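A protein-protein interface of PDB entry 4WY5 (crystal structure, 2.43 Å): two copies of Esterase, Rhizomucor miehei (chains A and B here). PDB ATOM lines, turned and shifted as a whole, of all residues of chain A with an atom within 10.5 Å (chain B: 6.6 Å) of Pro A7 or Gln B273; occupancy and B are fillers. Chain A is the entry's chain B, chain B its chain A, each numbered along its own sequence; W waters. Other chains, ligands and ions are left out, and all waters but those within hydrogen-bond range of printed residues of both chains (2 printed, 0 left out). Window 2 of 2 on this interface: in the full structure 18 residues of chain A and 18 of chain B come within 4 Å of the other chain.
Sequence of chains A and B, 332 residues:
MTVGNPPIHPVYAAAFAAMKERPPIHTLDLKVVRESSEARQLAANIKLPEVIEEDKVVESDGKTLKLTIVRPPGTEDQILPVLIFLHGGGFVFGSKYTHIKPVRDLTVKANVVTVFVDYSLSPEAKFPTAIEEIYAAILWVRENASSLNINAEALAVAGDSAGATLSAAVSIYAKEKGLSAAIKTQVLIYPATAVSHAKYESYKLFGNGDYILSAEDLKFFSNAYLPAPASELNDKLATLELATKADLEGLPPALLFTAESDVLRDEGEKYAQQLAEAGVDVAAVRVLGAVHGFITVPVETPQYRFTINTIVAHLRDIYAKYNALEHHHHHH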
ATOM      1  N   GLY A   4     -22.187  16.654 -30.916  1.00  0.00           N
ATOM      2  CA  GLY A   4     -20.826  16.487 -31.411  1.00  0.00           C
ATOM      3  C   GLY A   4     -19.843  17.383 -30.688  1.00  0.00           C
ATOM      4  O   GLY A   4     -18.633  17.364 -30.959  1.00  0.00           O
ATOM      5  N   ASN A   5     -20.373  18.142 -29.732  1.00  0.00           N
ATOM      6  CA  ASN A   5     -19.626  19.217 -29.102  1.00  0.00           C
ATOM      7  C   ASN A   5     -19.815  19.476 -27.585  1.00  0.00           C
ATOM      8  O   ASN A   5     -19.529  20.584 -27.135  1.00  0.00           O
ATOM      9  CB  ASN A   5     -19.935  20.516 -29.863  1.00  0.00           C
ATOM     10  CG  ASN A   5     -21.430  20.765 -30.016  1.00  0.00           C
ATOM     11  OD1 ASN A   5     -22.247  20.066 -29.421  1.00  0.00           O
ATOM     12  ND2 ASN A   5     -21.792  21.777 -30.814  1.00  0.00           N
ATOM     13  N   PRO A   6     -20.262  18.479 -26.783  1.00  0.00           N
ATOM     14  CA  PRO A   6     -20.169  18.833 -25.352  1.00  0.00           C
ATOM     15  C   PRO A   6     -18.722  18.903 -24.831  1.00  0.00           C
ATOM     16  O   PRO A   6     -17.802  18.345 -25.453  1.00  0.00           O
ATOM     17  CB  PRO A   6     -20.933  17.694 -24.649  1.00  0.00           C
ATOM     18  CG  PRO A   6     -20.865  16.542 -25.613  1.00  0.00           C
ATOM     19  CD  PRO A   6     -20.942  17.185 -26.980  1.00  0.00           C
ATOM     20  N   PRO A   7     -18.527  19.585 -23.693  1.00  0.00           N
ATOM     21  CA  PRO A   7     -17.234  19.616 -22.989  1.00  0.00           C
ATOM     22  C   PRO A   7     -16.719  18.236 -22.566  1.00  0.00           C
ATOM     23  O   PRO A   7     -17.518  17.326 -22.320  1.00  0.00           O
ATOM     24  CB  PRO A   7     -17.528  20.467 -21.739  1.00  0.00           C
ATOM     25  CG  PRO A   7     -18.742  21.305 -22.108  1.00  0.00           C
ATOM     26  CD  PRO A   7     -19.536  20.478 -23.079  1.00  0.00           C
ATOM     27  N   ILE A   8     -15.398  18.078 -22.549  1.00  0.00           N
ATOM     28  CA  ILE A   8     -14.746  16.918 -21.943  1.00  0.00           C
ATOM     29  C   ILE A   8     -13.848  17.425 -20.808  1.00  0.00           C
ATOM     30  O   ILE A   8     -13.505  18.612 -20.782  1.00  0.00           O
ATOM     31  CB  ILE A   8     -13.916  16.108 -22.967  1.00  0.00           C
ATOM     32  CG1 ILE A   8     -12.850  17.001 -23.615  1.00  0.00           C
ATOM     33  CG2 ILE A   8     -14.820  15.516 -24.040  1.00  0.00           C
ATOM     34  CD1 ILE A   8     -11.924  16.267 -24.564  1.00  0.00           C
ATOM     35  N   HIS A   9     -13.487  16.550 -19.869  1.00  0.00           N
ATOM     36  CA  HIS A   9     -12.602  16.930 -18.759  1.00  0.00           C
ATOM     37  C   HIS A   9     -11.204  17.315 -19.273  1.00  0.00           C
ATOM     38  O   HIS A   9     -10.656  16.638 -20.153  1.00  0.00           O
ATOM     39  CB  HIS A   9     -12.510  15.793 -17.742  1.00  0.00           C
ATOM     40  CG  HIS A   9     -11.929  16.204 -16.424  1.00  0.00           C
ATOM     41  ND1 HIS A   9     -10.590  16.468 -16.250  1.00  0.00           N
ATOM     42  CD2 HIS A   9     -12.512  16.394 -15.211  1.00  0.00           C
ATOM     43  CE1 HIS A   9     -10.365  16.796 -14.984  1.00  0.00           C
ATOM     44  NE2 HIS A   9     -11.516  16.767 -14.339  1.00  0.00           N
ATOM     45  N   PRO A  10     -10.629  18.409 -18.731  1.00  0.00           N
ATOM     46  CA  PRO A  10      -9.316  18.920 -19.169  1.00  0.00           C
ATOM     47  C   PRO A  10      -8.260  17.826 -19.231  1.00  0.00           C
ATOM     48  O   PRO A  10      -7.411  17.853 -20.123  1.00  0.00           O
ATOM     49  CB  PRO A  10      -8.959  19.960 -18.095  1.00  0.00           C
ATOM     50  CG  PRO A  10     -10.291  20.454 -17.600  1.00  0.00           C
ATOM     51  CD  PRO A  10     -11.257  19.283 -17.717  1.00  0.00           C
ATOM     52  N   VAL A  11      -8.321  16.878 -18.297  1.00  0.00           N
ATOM     53  CA  VAL A  11      -7.398  15.744 -18.268  1.00  0.00           C
ATOM     54  C   VAL A  11      -7.516  14.863 -19.520  1.00  0.00           C
ATOM     55  O   VAL A  11      -6.502  14.373 -20.026  1.00  0.00           O
ATOM     56  CB  VAL A  11      -7.617  14.882 -16.980  1.00  0.00           C
ATOM     57  CG1 VAL A  11      -7.047  13.469 -17.132  1.00  0.00           C
ATOM     58  CG2 VAL A  11      -6.981  15.554 -15.783  1.00  0.00           C
ATOM     59  N   TYR A  12      -8.734  14.668 -20.032  1.00  0.00           N
ATOM     60  CA  TYR A  12      -8.921  13.821 -21.216  1.00  0.00           C
ATOM     61  C   TYR A  12      -8.482  14.521 -22.489  1.00  0.00           C
ATOM     62  O   TYR A  12      -8.006  13.877 -23.425  1.00  0.00           O
ATOM     63  CB  TYR A  12     -10.376  13.350 -21.349  1.00  0.00           C
ATOM     64  CG  TYR A  12     -10.829  12.501 -20.179  1.00  0.00           C
ATOM     65  CD1 TYR A  12      -9.975  11.566 -19.601  1.00  0.00           C
ATOM     66  CD2 TYR A  12     -12.102  12.649 -19.641  1.00  0.00           C
ATOM     67  CE1 TYR A  12     -10.379  10.798 -18.522  1.00  0.00           C
ATOM     68  CE2 TYR A  12     -12.517  11.895 -18.565  1.00  0.00           C
ATOM     69  CZ  TYR A  12     -11.660  10.969 -18.003  1.00  0.00           C
ATOM     70  OH  TYR A  12     -12.092  10.219 -16.920  1.00  0.00           O
ATOM     71  N   ALA A  13      -8.668  15.834 -22.545  1.00  0.00           N
ATOM     72  CA  ALA A  13      -8.196  16.611 -23.694  1.00  0.00           C
ATOM     73  C   ALA A  13      -6.658  16.552 -23.766  1.00  0.00           C
ATOM     74  O   ALA A  13      -6.074  16.414 -24.846  1.00  0.00           O
ATOM     75  CB  ALA A  13      -8.679  18.058 -23.600  1.00  0.00           C
ATOM     76  N   PHE A 206     -18.108  11.939 -33.308  1.00  0.00           N
ATOM     77  CA  PHE A 206     -16.824  11.819 -32.606  1.00  0.00           C
ATOM     78  C   PHE A 206     -15.785  10.977 -33.343  1.00  0.00           C
ATOM     79  O   PHE A 206     -14.738  10.648 -32.771  1.00  0.00           O
ATOM     80  CB  PHE A 206     -17.049  11.237 -31.192  1.00  0.00           C
ATOM     81  CG  PHE A 206     -18.169  11.917 -30.429  1.00  0.00           C
ATOM     82  CD1 PHE A 206     -18.048  13.242 -30.013  1.00  0.00           C
ATOM     83  CD2 PHE A 206     -19.341  11.227 -30.126  1.00  0.00           C
ATOM     84  CE1 PHE A 206     -19.082  13.877 -29.317  1.00  0.00           C
ATOM     85  CE2 PHE A 206     -20.385  11.856 -29.429  1.00  0.00           C
ATOM     86  CZ  PHE A 206     -20.255  13.186 -29.028  1.00  0.00           C
ATOM     87  N   TYR A 211     -11.105  12.867 -31.637  1.00  0.00           N
ATOM     88  CA  TYR A 211     -11.269  12.137 -30.359  1.00  0.00           C
ATOM     89  C   TYR A 211     -10.493  10.810 -30.324  1.00  0.00           C
ATOM     90  O   TYR A 211     -10.099  10.276 -31.368  1.00  0.00           O
ATOM     91  CB  TYR A 211     -12.758  11.873 -30.061  1.00  0.00           C
ATOM     92  CG  TYR A 211     -13.568  13.138 -29.846  1.00  0.00           C
ATOM     93  CD1 TYR A 211     -14.120  13.830 -30.934  1.00  0.00           C
ATOM     94  CD2 TYR A 211     -13.771  13.654 -28.568  1.00  0.00           C
ATOM     95  CE1 TYR A 211     -14.864  14.989 -30.755  1.00  0.00           C
ATOM     96  CE2 TYR A 211     -14.520  14.821 -28.372  1.00  0.00           C
ATOM     97  CZ  TYR A 211     -15.061  15.483 -29.479  1.00  0.00           C
ATOM     98  OH  TYR A 211     -15.800  16.644 -29.321  1.00  0.00           O
ATOM     99  N   ALA A 259     -19.683   6.055 -22.614  1.00  0.00           N
ATOM    100  CA  ALA A 259     -19.017   7.351 -22.488  1.00  0.00           C
ATOM    101  C   ALA A 259     -19.661   8.398 -23.404  1.00  0.00           C
ATOM    102  O   ALA A 259     -19.954   8.103 -24.567  1.00  0.00           O
ATOM    103  CB  ALA A 259     -17.519   7.216 -22.802  1.00  0.00           C
ATOM    104  N   GLU A 260     -19.874   9.612 -22.887  1.00  0.00           N
ATOM    105  CA  GLU A 260     -20.596  10.636 -23.638  1.00  0.00           C
ATOM    106  C   GLU A 260     -19.930  10.970 -24.970  1.00  0.00           C
ATOM    107  O   GLU A 260     -20.618  11.056 -25.992  1.00  0.00           O
ATOM    108  CB  GLU A 260     -20.763  11.926 -22.820  1.00  0.00           C
ATOM    109  CG  GLU A 260     -21.505  13.029 -23.605  1.00  0.00           C
ATOM    110  CD  GLU A 260     -21.758  14.301 -22.802  1.00  0.00           C
ATOM    111  OE1 GLU A 260     -20.817  14.786 -22.123  1.00  0.00           O
ATOM    112  OE2 GLU A 260     -22.909  14.808 -22.844  1.00  0.00           O
ATOM    113  N   SER A 261     -18.608  11.170 -24.973  1.00  0.00           N
ATOM    114  CA  SER A 261     -17.917  11.526 -26.218  1.00  0.00           C
ATOM    115  C   SER A 261     -17.116  10.349 -26.761  1.00  0.00           C
ATOM    116  O   SER A 261     -15.892  10.295 -26.634  1.00  0.00           O
ATOM    117  CB  SER A 261     -17.005  12.745 -26.014  1.00  0.00           C
ATOM    118  OG  SER A 261     -17.758  13.944 -25.809  1.00  0.00           O
ATOM    119  N   ASP A 262     -17.820   9.436 -27.422  1.00  0.00           N
ATOM    120  CA  ASP A 262     -17.285   8.134 -27.816  1.00  0.00           C
ATOM    121  C   ASP A 262     -18.126   7.586 -28.970  1.00  0.00           C
ATOM    122  O   ASP A 262     -19.353   7.462 -28.842  1.00  0.00           O
ATOM    123  CB  ASP A 262     -17.303   7.187 -26.608  1.00  0.00           C
ATOM    124  CG  ASP A 262     -16.743   5.788 -26.917  1.00  0.00           C
ATOM    125  OD1 ASP A 262     -16.444   5.492 -28.099  1.00  0.00           O
ATOM    126  OD2 ASP A 262     -16.605   4.971 -25.952  1.00  0.00           O
ATOM    127  N   ARG A 265     -20.845   5.049 -28.360  1.00  0.00           N
ATOM    128  CA  ARG A 265     -21.837   5.405 -27.335  1.00  0.00           C
ATOM    129  C   ARG A 265     -23.221   4.838 -27.627  1.00  0.00           C
ATOM    130  O   ARG A 265     -23.798   4.131 -26.790  1.00  0.00           O
ATOM    131  CB  ARG A 265     -21.939   6.932 -27.182  1.00  0.00           C
ATOM    132  CG  ARG A 265     -22.898   7.421 -26.087  1.00  0.00           C
ATOM    133  CD  ARG A 265     -23.004   8.941 -26.123  1.00  0.00           C
ATOM    134  NE  ARG A 265     -23.933   9.385 -27.158  1.00  0.00           N
ATOM    135  CZ  ARG A 265     -24.030  10.637 -27.598  1.00  0.00           C
ATOM    136  NH1 ARG A 265     -23.240  11.580 -27.113  1.00  0.00           N
ATOM    137  NH2 ARG A 265     -24.914  10.944 -28.537  1.00  0.00           N
ATOM    138  N   ARG A 286     -24.981   6.683 -18.959  1.00  0.00           N
ATOM    139  CA  ARG A 286     -24.045   7.467 -19.780  1.00  0.00           C
ATOM    140  C   ARG A 286     -23.197   8.398 -18.898  1.00  0.00           C
ATOM    141  O   ARG A 286     -23.738   9.206 -18.120  1.00  0.00           O
ATOM    142  CB  ARG A 286     -24.796   8.295 -20.836  1.00  0.00           C
ATOM    143  CG  ARG A 286     -23.892   9.171 -21.734  1.00  0.00           C
ATOM    144  CD  ARG A 286     -24.699  10.180 -22.632  1.00  0.00           C
ATOM    145  NE  ARG A 286     -25.498   9.470 -23.632  1.00  0.00           N
ATOM    146  CZ  ARG A 286     -26.174  10.030 -24.634  1.00  0.00           C
ATOM    147  NH1 ARG A 286     -26.158  11.349 -24.824  1.00  0.00           N
ATOM    148  NH2 ARG A 286     -26.863   9.255 -25.464  1.00  0.00           N
ATOM    149  N   VAL A 287     -21.872   8.284 -19.000  1.00  0.00           N
ATOM    150  CA  VAL A 287     -20.987   9.114 -18.167  1.00  0.00           C
ATOM    151  C   VAL A 287     -20.607  10.421 -18.863  1.00  0.00           C
ATOM    152  O   VAL A 287     -19.923  10.427 -19.896  1.00  0.00           O
ATOM    153  CB  VAL A 287     -19.698   8.351 -17.766  1.00  0.00           C
ATOM    154  CG1 VAL A 287     -18.839   9.193 -16.826  1.00  0.00           C
ATOM    155  CG2 VAL A 287     -20.054   6.999 -17.142  1.00  0.00           C
ATOM    156  N   LEU A 288     -21.036  11.529 -18.261  1.00  0.00           N
ATOM    157  CA  LEU A 288     -20.880  12.882 -18.821  1.00  0.00           C
ATOM    158  C   LEU A 288     -19.463  13.414 -18.669  1.00  0.00           C
ATOM    159  O   LEU A 288     -18.833  13.243 -17.614  1.00  0.00           O
ATOM    160  CB  LEU A 288     -21.883  13.823 -18.134  1.00  0.00           C
ATOM    161  CG  LEU A 288     -23.259  13.947 -18.809  1.00  0.00           C
ATOM    162  CD1 LEU A 288     -23.711  12.642 -19.444  1.00  0.00           C
ATOM    163  CD2 LEU A 288     -24.292  14.326 -17.780  1.00  0.00           C
ATOM    164  N   GLY A 289     -18.953  14.031 -19.734  1.00  0.00           N
ATOM    165  CA  GLY A 289     -17.618  14.607 -19.731  1.00  0.00           C
ATOM    166  C   GLY A 289     -16.509  13.605 -20.062  1.00  0.00           C
ATOM    167  O   GLY A 289     -15.322  13.970 -20.113  1.00  0.00           O
ATOM    168  N   ALA A 290     -16.881  12.347 -20.294  1.00  0.00           N
ATOM    169  CA  ALA A 290     -15.873  11.301 -20.456  1.00  0.00           C
ATOM    170  C   ALA A 290     -15.679  10.899 -21.912  1.00  0.00           C
ATOM    171  O   ALA A 290     -16.555  11.146 -22.754  1.00  0.00           O
ATOM    172  CB  ALA A 290     -16.231  10.075 -19.612  1.00  0.00           C
ATOM    173  N   VAL A 291     -14.517  10.299 -22.200  1.00  0.00           N
ATOM    174  CA  VAL A 291     -14.163   9.844 -23.557  1.00  0.00           C
ATOM    175  C   VAL A 291     -13.913   8.339 -23.553  1.00  0.00           C
ATOM    176  O   VAL A 291     -13.746   7.733 -22.490  1.00  0.00           O
ATOM    177  CB  VAL A 291     -12.896  10.536 -24.073  1.00  0.00           C
ATOM    178  CG1 VAL A 291     -13.100  12.038 -24.084  1.00  0.00           C
ATOM    179  CG2 VAL A 291     -11.710  10.196 -23.164  1.00  0.00           C
ATOM    180  N   GLN A 303     -14.648  11.153 -12.648  1.00  0.00           N
ATOM    181  CA  GLN A 303     -15.264  10.052 -13.380  1.00  0.00           C
ATOM    182  C   GLN A 303     -14.543   8.711 -13.148  1.00  0.00           C
ATOM    183  O   GLN A 303     -15.190   7.654 -13.139  1.00  0.00           O
ATOM    184  CB  GLN A 303     -15.261  10.336 -14.907  1.00  0.00           C
ATOM    185  CG  GLN A 303     -16.137  11.489 -15.394  1.00  0.00           C
ATOM    186  CD  GLN A 303     -15.384  12.806 -15.488  1.00  0.00           C
ATOM    187  OE1 GLN A 303     -14.413  13.017 -14.772  1.00  0.00           O
ATOM    188  NE2 GLN A 303     -15.828  13.695 -16.381  1.00  0.00           N
ATOM    189  N   ASP B 266     -32.052  17.531 -20.078  1.00  0.00           N
ATOM    190  CA  ASP B 266     -30.963  18.239 -20.725  1.00  0.00           C
ATOM    191  C   ASP B 266     -30.527  19.453 -19.907  1.00  0.00           C
ATOM    192  O   ASP B 266     -29.359  19.835 -19.925  1.00  0.00           O
ATOM    193  CB  ASP B 266     -31.379  18.700 -22.138  1.00  0.00           C
ATOM    194  CG  ASP B 266     -31.618  17.545 -23.109  1.00  0.00           C
ATOM    195  OD1 ASP B 266     -31.300  16.389 -22.771  1.00  0.00           O
ATOM    196  OD2 ASP B 266     -32.123  17.803 -24.229  1.00  0.00           O
ATOM    197  N   GLY B 268     -30.684  19.531 -16.699  1.00  0.00           N
ATOM    198  CA  GLY B 268     -29.917  18.931 -15.636  1.00  0.00           C
ATOM    199  C   GLY B 268     -28.489  18.669 -16.089  1.00  0.00           C
ATOM    200  O   GLY B 268     -27.540  18.948 -15.351  1.00  0.00           O
ATOM    201  N   GLU B 269     -28.321  18.151 -17.305  1.00  0.00           N
ATOM    202  CA  GLU B 269     -26.975  17.821 -17.776  1.00  0.00           C
ATOM    203  C   GLU B 269     -26.196  19.115 -18.054  1.00  0.00           C
ATOM    204  O   GLU B 269     -24.978  19.162 -17.889  1.00  0.00           O
ATOM    205  CB  GLU B 269     -27.028  16.919 -19.032  1.00  0.00           C
ATOM    206  CG  GLU B 269     -27.768  15.586 -18.809  1.00  0.00           C
ATOM    207  CD  GLU B 269     -27.722  14.621 -19.992  1.00  0.00           C
ATOM    208  OE1 GLU B 269     -27.101  14.934 -21.042  1.00  0.00           O
ATOM    209  OE2 GLU B 269     -28.333  13.525 -19.875  1.00  0.00           O
ATOM    210  N   LYS B 270     -26.904  20.191 -18.384  1.00  0.00           N
ATOM    211  CA  LYS B 270     -26.232  21.468 -18.635  1.00  0.00           C
ATOM    212  C   LYS B 270     -25.674  22.041 -17.338  1.00  0.00           C
ATOM    213  O   LYS B 270     -24.578  22.577 -17.326  1.00  0.00           O
ATOM    214  CB  LYS B 270     -27.180  22.467 -19.288  1.00  0.00           C
ATOM    215  CG  LYS B 270     -26.594  23.870 -19.474  1.00  0.00           C
ATOM    216  CD  LYS B 270     -25.562  23.934 -20.594  1.00  0.00           C
ATOM    217  CE  LYS B 270     -24.971  25.347 -20.701  1.00  0.00           C
ATOM    218  NZ  LYS B 270     -24.324  25.591 -22.029  1.00  0.00           N
ATOM    219  N   TYR B 271     -26.394  21.882 -16.236  1.00  0.00           N
ATOM    220  CA  TYR B 271     -25.888  22.370 -14.944  1.00  0.00           C
ATOM    221  C   TYR B 271     -24.631  21.604 -14.507  1.00  0.00           C
ATOM    222  O   TYR B 271     -23.703  22.186 -13.934  1.00  0.00           O
ATOM    223  CB  TYR B 271     -26.979  22.272 -13.856  1.00  0.00           C
ATOM    224  CG  TYR B 271     -26.660  23.002 -12.557  1.00  0.00           C
ATOM    225  CD1 TYR B 271     -26.590  24.396 -12.512  1.00  0.00           C
ATOM    226  CD2 TYR B 271     -26.430  22.297 -11.377  1.00  0.00           C
ATOM    227  CE1 TYR B 271     -26.298  25.069 -11.327  1.00  0.00           C
ATOM    228  CE2 TYR B 271     -26.139  22.952 -10.189  1.00  0.00           C
ATOM    229  CZ  TYR B 271     -26.074  24.343 -10.164  1.00  0.00           C
ATOM    230  OH  TYR B 271     -25.779  25.004  -8.981  1.00  0.00           O
ATOM    231  N   ALA B 272     -24.582  20.305 -14.796  1.00  0.00           N
ATOM    232  CA  ALA B 272     -23.370  19.520 -14.531  1.00  0.00           C
ATOM    233  C   ALA B 272     -22.162  20.135 -15.249  1.00  0.00           C
ATOM    234  O   ALA B 272     -21.074  20.248 -14.681  1.00  0.00           O
ATOM    235  CB  ALA B 272     -23.568  18.055 -14.964  1.00  0.00           C
ATOM    236  N   GLN B 273     -22.370  20.518 -16.503  1.00  0.00           N
ATOM    237  CA  GLN B 273     -21.333  21.145 -17.316  1.00  0.00           C
ATOM    238  C   GLN B 273     -20.874  22.489 -16.729  1.00  0.00           C
ATOM    239  O   GLN B 273     -19.681  22.804 -16.747  1.00  0.00           O
ATOM    240  CB  GLN B 273     -21.837  21.347 -18.755  1.00  0.00           C
ATOM    241  CG  GLN B 273     -22.227  20.062 -19.494  1.00  0.00           C
ATOM    242  CD  GLN B 273     -22.749  20.318 -20.917  1.00  0.00           C
ATOM    243  OE1 GLN B 273     -22.681  21.436 -21.435  1.00  0.00           O
ATOM    244  NE2 GLN B 273     -23.257  19.267 -21.557  1.00  0.00           N
ATOM    245  N   GLN B 274     -21.833  23.265 -16.217  1.00  0.00           N
ATOM    246  CA  GLN B 274     -21.576  24.567 -15.584  1.00  0.00           C
ATOM    247  C   GLN B 274     -20.709  24.424 -14.328  1.00  0.00           C
ATOM    248  O   GLN B 274     -19.771  25.205 -14.092  1.00  0.00           O
ATOM    249  CB  GLN B 274     -22.898  25.258 -15.188  1.00  0.00           C
ATOM    250  CG  GLN B 274     -23.887  25.549 -16.327  1.00  0.00           C
ATOM    251  CD  GLN B 274     -25.170  26.247 -15.843  1.00  0.00           C
ATOM    252  OE1 GLN B 274     -26.284  25.730 -16.007  1.00  0.00           O
ATOM    253  NE2 GLN B 274     -25.011  27.426 -15.241  1.00  0.00           N
ATOM    254  N   LEU B 275     -21.015  23.412 -13.521  1.00  0.00           N
ATOM    255  CA  LEU B 275     -20.233  23.173 -12.315  1.00  0.00           C
ATOM    256  C   LEU B 275     -18.796  22.790 -12.680  1.00  0.00           C
ATOM    257  O   LEU B 275     -17.847  23.313 -12.093  1.00  0.00           O
ATOM    258  CB  LEU B 275     -20.887  22.084 -11.457  1.00  0.00           C
ATOM    259  CG  LEU B 275     -22.213  22.408 -10.758  1.00  0.00           C
ATOM    260  CD1 LEU B 275     -22.922  21.120 -10.400  1.00  0.00           C
ATOM    261  CD2 LEU B 275     -22.020  23.251  -9.487  1.00  0.00           C
ATOM    262  N   ALA B 276     -18.619  21.949 -13.693  1.00  0.00           N
ATOM    263  CA  ALA B 276     -17.260  21.540 -14.068  1.00  0.00           C
ATOM    264  C   ALA B 276     -16.423  22.696 -14.644  1.00  0.00           C
ATOM    265  O   ALA B 276     -15.224  22.803 -14.385  1.00  0.00           O
ATOM    266  CB  ALA B 276     -17.319  20.373 -15.067  1.00  0.00           C
ATOM    267  N   GLU B 277     -17.062  23.583 -15.394  1.00  0.00           N
ATOM    268  CA  GLU B 277     -16.383  24.760 -15.934  1.00  0.00           C
ATOM    269  C   GLU B 277     -15.850  25.673 -14.817  1.00  0.00           C
ATOM    270  O   GLU B 277     -14.825  26.340 -14.975  1.00  0.00           O
ATOM    271  CB  GLU B 277     -17.333  25.527 -16.857  1.00  0.00           C
ATOM    272  CG  GLU B 277     -16.833  26.896 -17.308  1.00  0.00           C
ATOM    273  CD  GLU B 277     -17.923  27.734 -17.981  1.00  0.00           C
ATOM    274  OE1 GLU B 277     -17.775  28.978 -18.040  1.00  0.00           O
ATOM    275  OE2 GLU B 277     -18.940  27.155 -18.423  1.00  0.00           O
ATOM    276  N   ALA B 278     -16.542  25.686 -13.683  1.00  0.00           N
ATOM    277  CA  ALA B 278     -16.151  26.528 -12.563  1.00  0.00           C
ATOM    278  C   ALA B 278     -15.152  25.827 -11.661  1.00  0.00           C
ATOM    279  O   ALA B 278     -14.781  26.360 -10.614  1.00  0.00           O
ATOM    280  CB  ALA B 278     -17.378  26.946 -11.757  1.00  0.00           C
ATOM    281  N   VAL B 282     -17.303  17.083 -10.244  1.00  0.00           N
ATOM    282  CA  VAL B 282     -18.640  16.607 -10.632  1.00  0.00           C
ATOM    283  C   VAL B 282     -18.621  15.201 -11.249  1.00  0.00           C
ATOM    284  O   VAL B 282     -17.869  14.940 -12.194  1.00  0.00           O
ATOM    285  CB  VAL B 282     -19.306  17.569 -11.652  1.00  0.00           C
ATOM    286  CG1 VAL B 282     -20.702  17.077 -12.043  1.00  0.00           C
ATOM    287  CG2 VAL B 282     -19.382  18.954 -11.076  1.00  0.00           C
ATOM    288  N   ALA B 284     -21.462  12.922 -13.006  1.00  0.00           N
ATOM    289  CA  ALA B 284     -22.812  13.051 -13.540  1.00  0.00           C
ATOM    290  C   ALA B 284     -23.104  11.903 -14.499  1.00  0.00           C
ATOM    291  O   ALA B 284     -22.241  11.548 -15.304  1.00  0.00           O
ATOM    292  CB  ALA B 284     -22.970  14.406 -14.257  1.00  0.00           C
HETATM  293  O   HOH W   1     -25.465  13.776 -22.853  1.00  0.00           O
HETATM  294  O   HOH W   2     -19.060  13.122 -15.093  1.00  0.00           O
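O of Leu A288 is in hydrogen-bond range of NE2 of Gln A303 (3.3 Å).
N of Glu A260 lies within hydrogen-bond range of O of Val A287.
Water W2 bridges the backbone carbonyl oxygen of Leu A288 (2.5 Å) and the backbone NH of Ala B284 (3.2 Å).
Water W1 lies within hydrogen-bond range of the side-chain carboxylate (OE1) of Glu B269 (2.7 Å), the side-chain carboxylate (OE2) of Glu A260 (2.8 Å) and the guanidinium group (NH1) of Arg A286 (3.2 Å).
The backbone NH (N) of Leu A288 sits at hydrogen-bond distance from the backbone carbonyl oxygen (O) of Ala B284 (3.2 Å).
Pro A7 touches one residue of chain B.
Gln B273 touches just one residue of chain A: Pro A7.
No residue of chain A comes within 4 Å of Ala B272.
No residue of chain A comes within 4 Å of Ala B276.
Printed residues of chain B within 4 Å of Arg A286: Ala B284 (3.96 Å).
Of the printed residues of chain A, Ala B284 touches Arg A286, Val A287 and Leu A288.
Of the printed residues of chain B, Val A287 touches Ala B284.
Of the printed residues of chain A, Glu B269 touches Leu A288.
The nearest printed residue of chain A that does not touch Ala B284 is Gln A303 (6.0 Å).
No position is printed for both chains.
Of the 5 pairs that touch across the chains among the printed residues, none has its exchanged pair printed and touching as well.
Among the printed residues, merely in contact across the chains: Pro A7 with Gln B273 (3.7 Å), Leu A288 with Glu B269 (3.8 Å), Arg A286 with Ala B284 (3.96 Å) and Val A287 with Ala B284 (3.96 Å).
Of the 14 printed residues of chain B, 3 touch a printed residue of chain A.
Printed residues of chain A that touch a printed residue of chain B: Pro A7, Arg A286, Val A287 and Leu A288.
Hydrophobic or aromatic side chains of chain A that line the printed part of chain B: Pro A7 and Leu A288.
Among the printed residues, 5 pairs touch across the chains.
Among the printed residues, no Asp or Glu carboxylate lies within 4 Å of a Lys or Arg side-chain nitrogen of the other chain.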
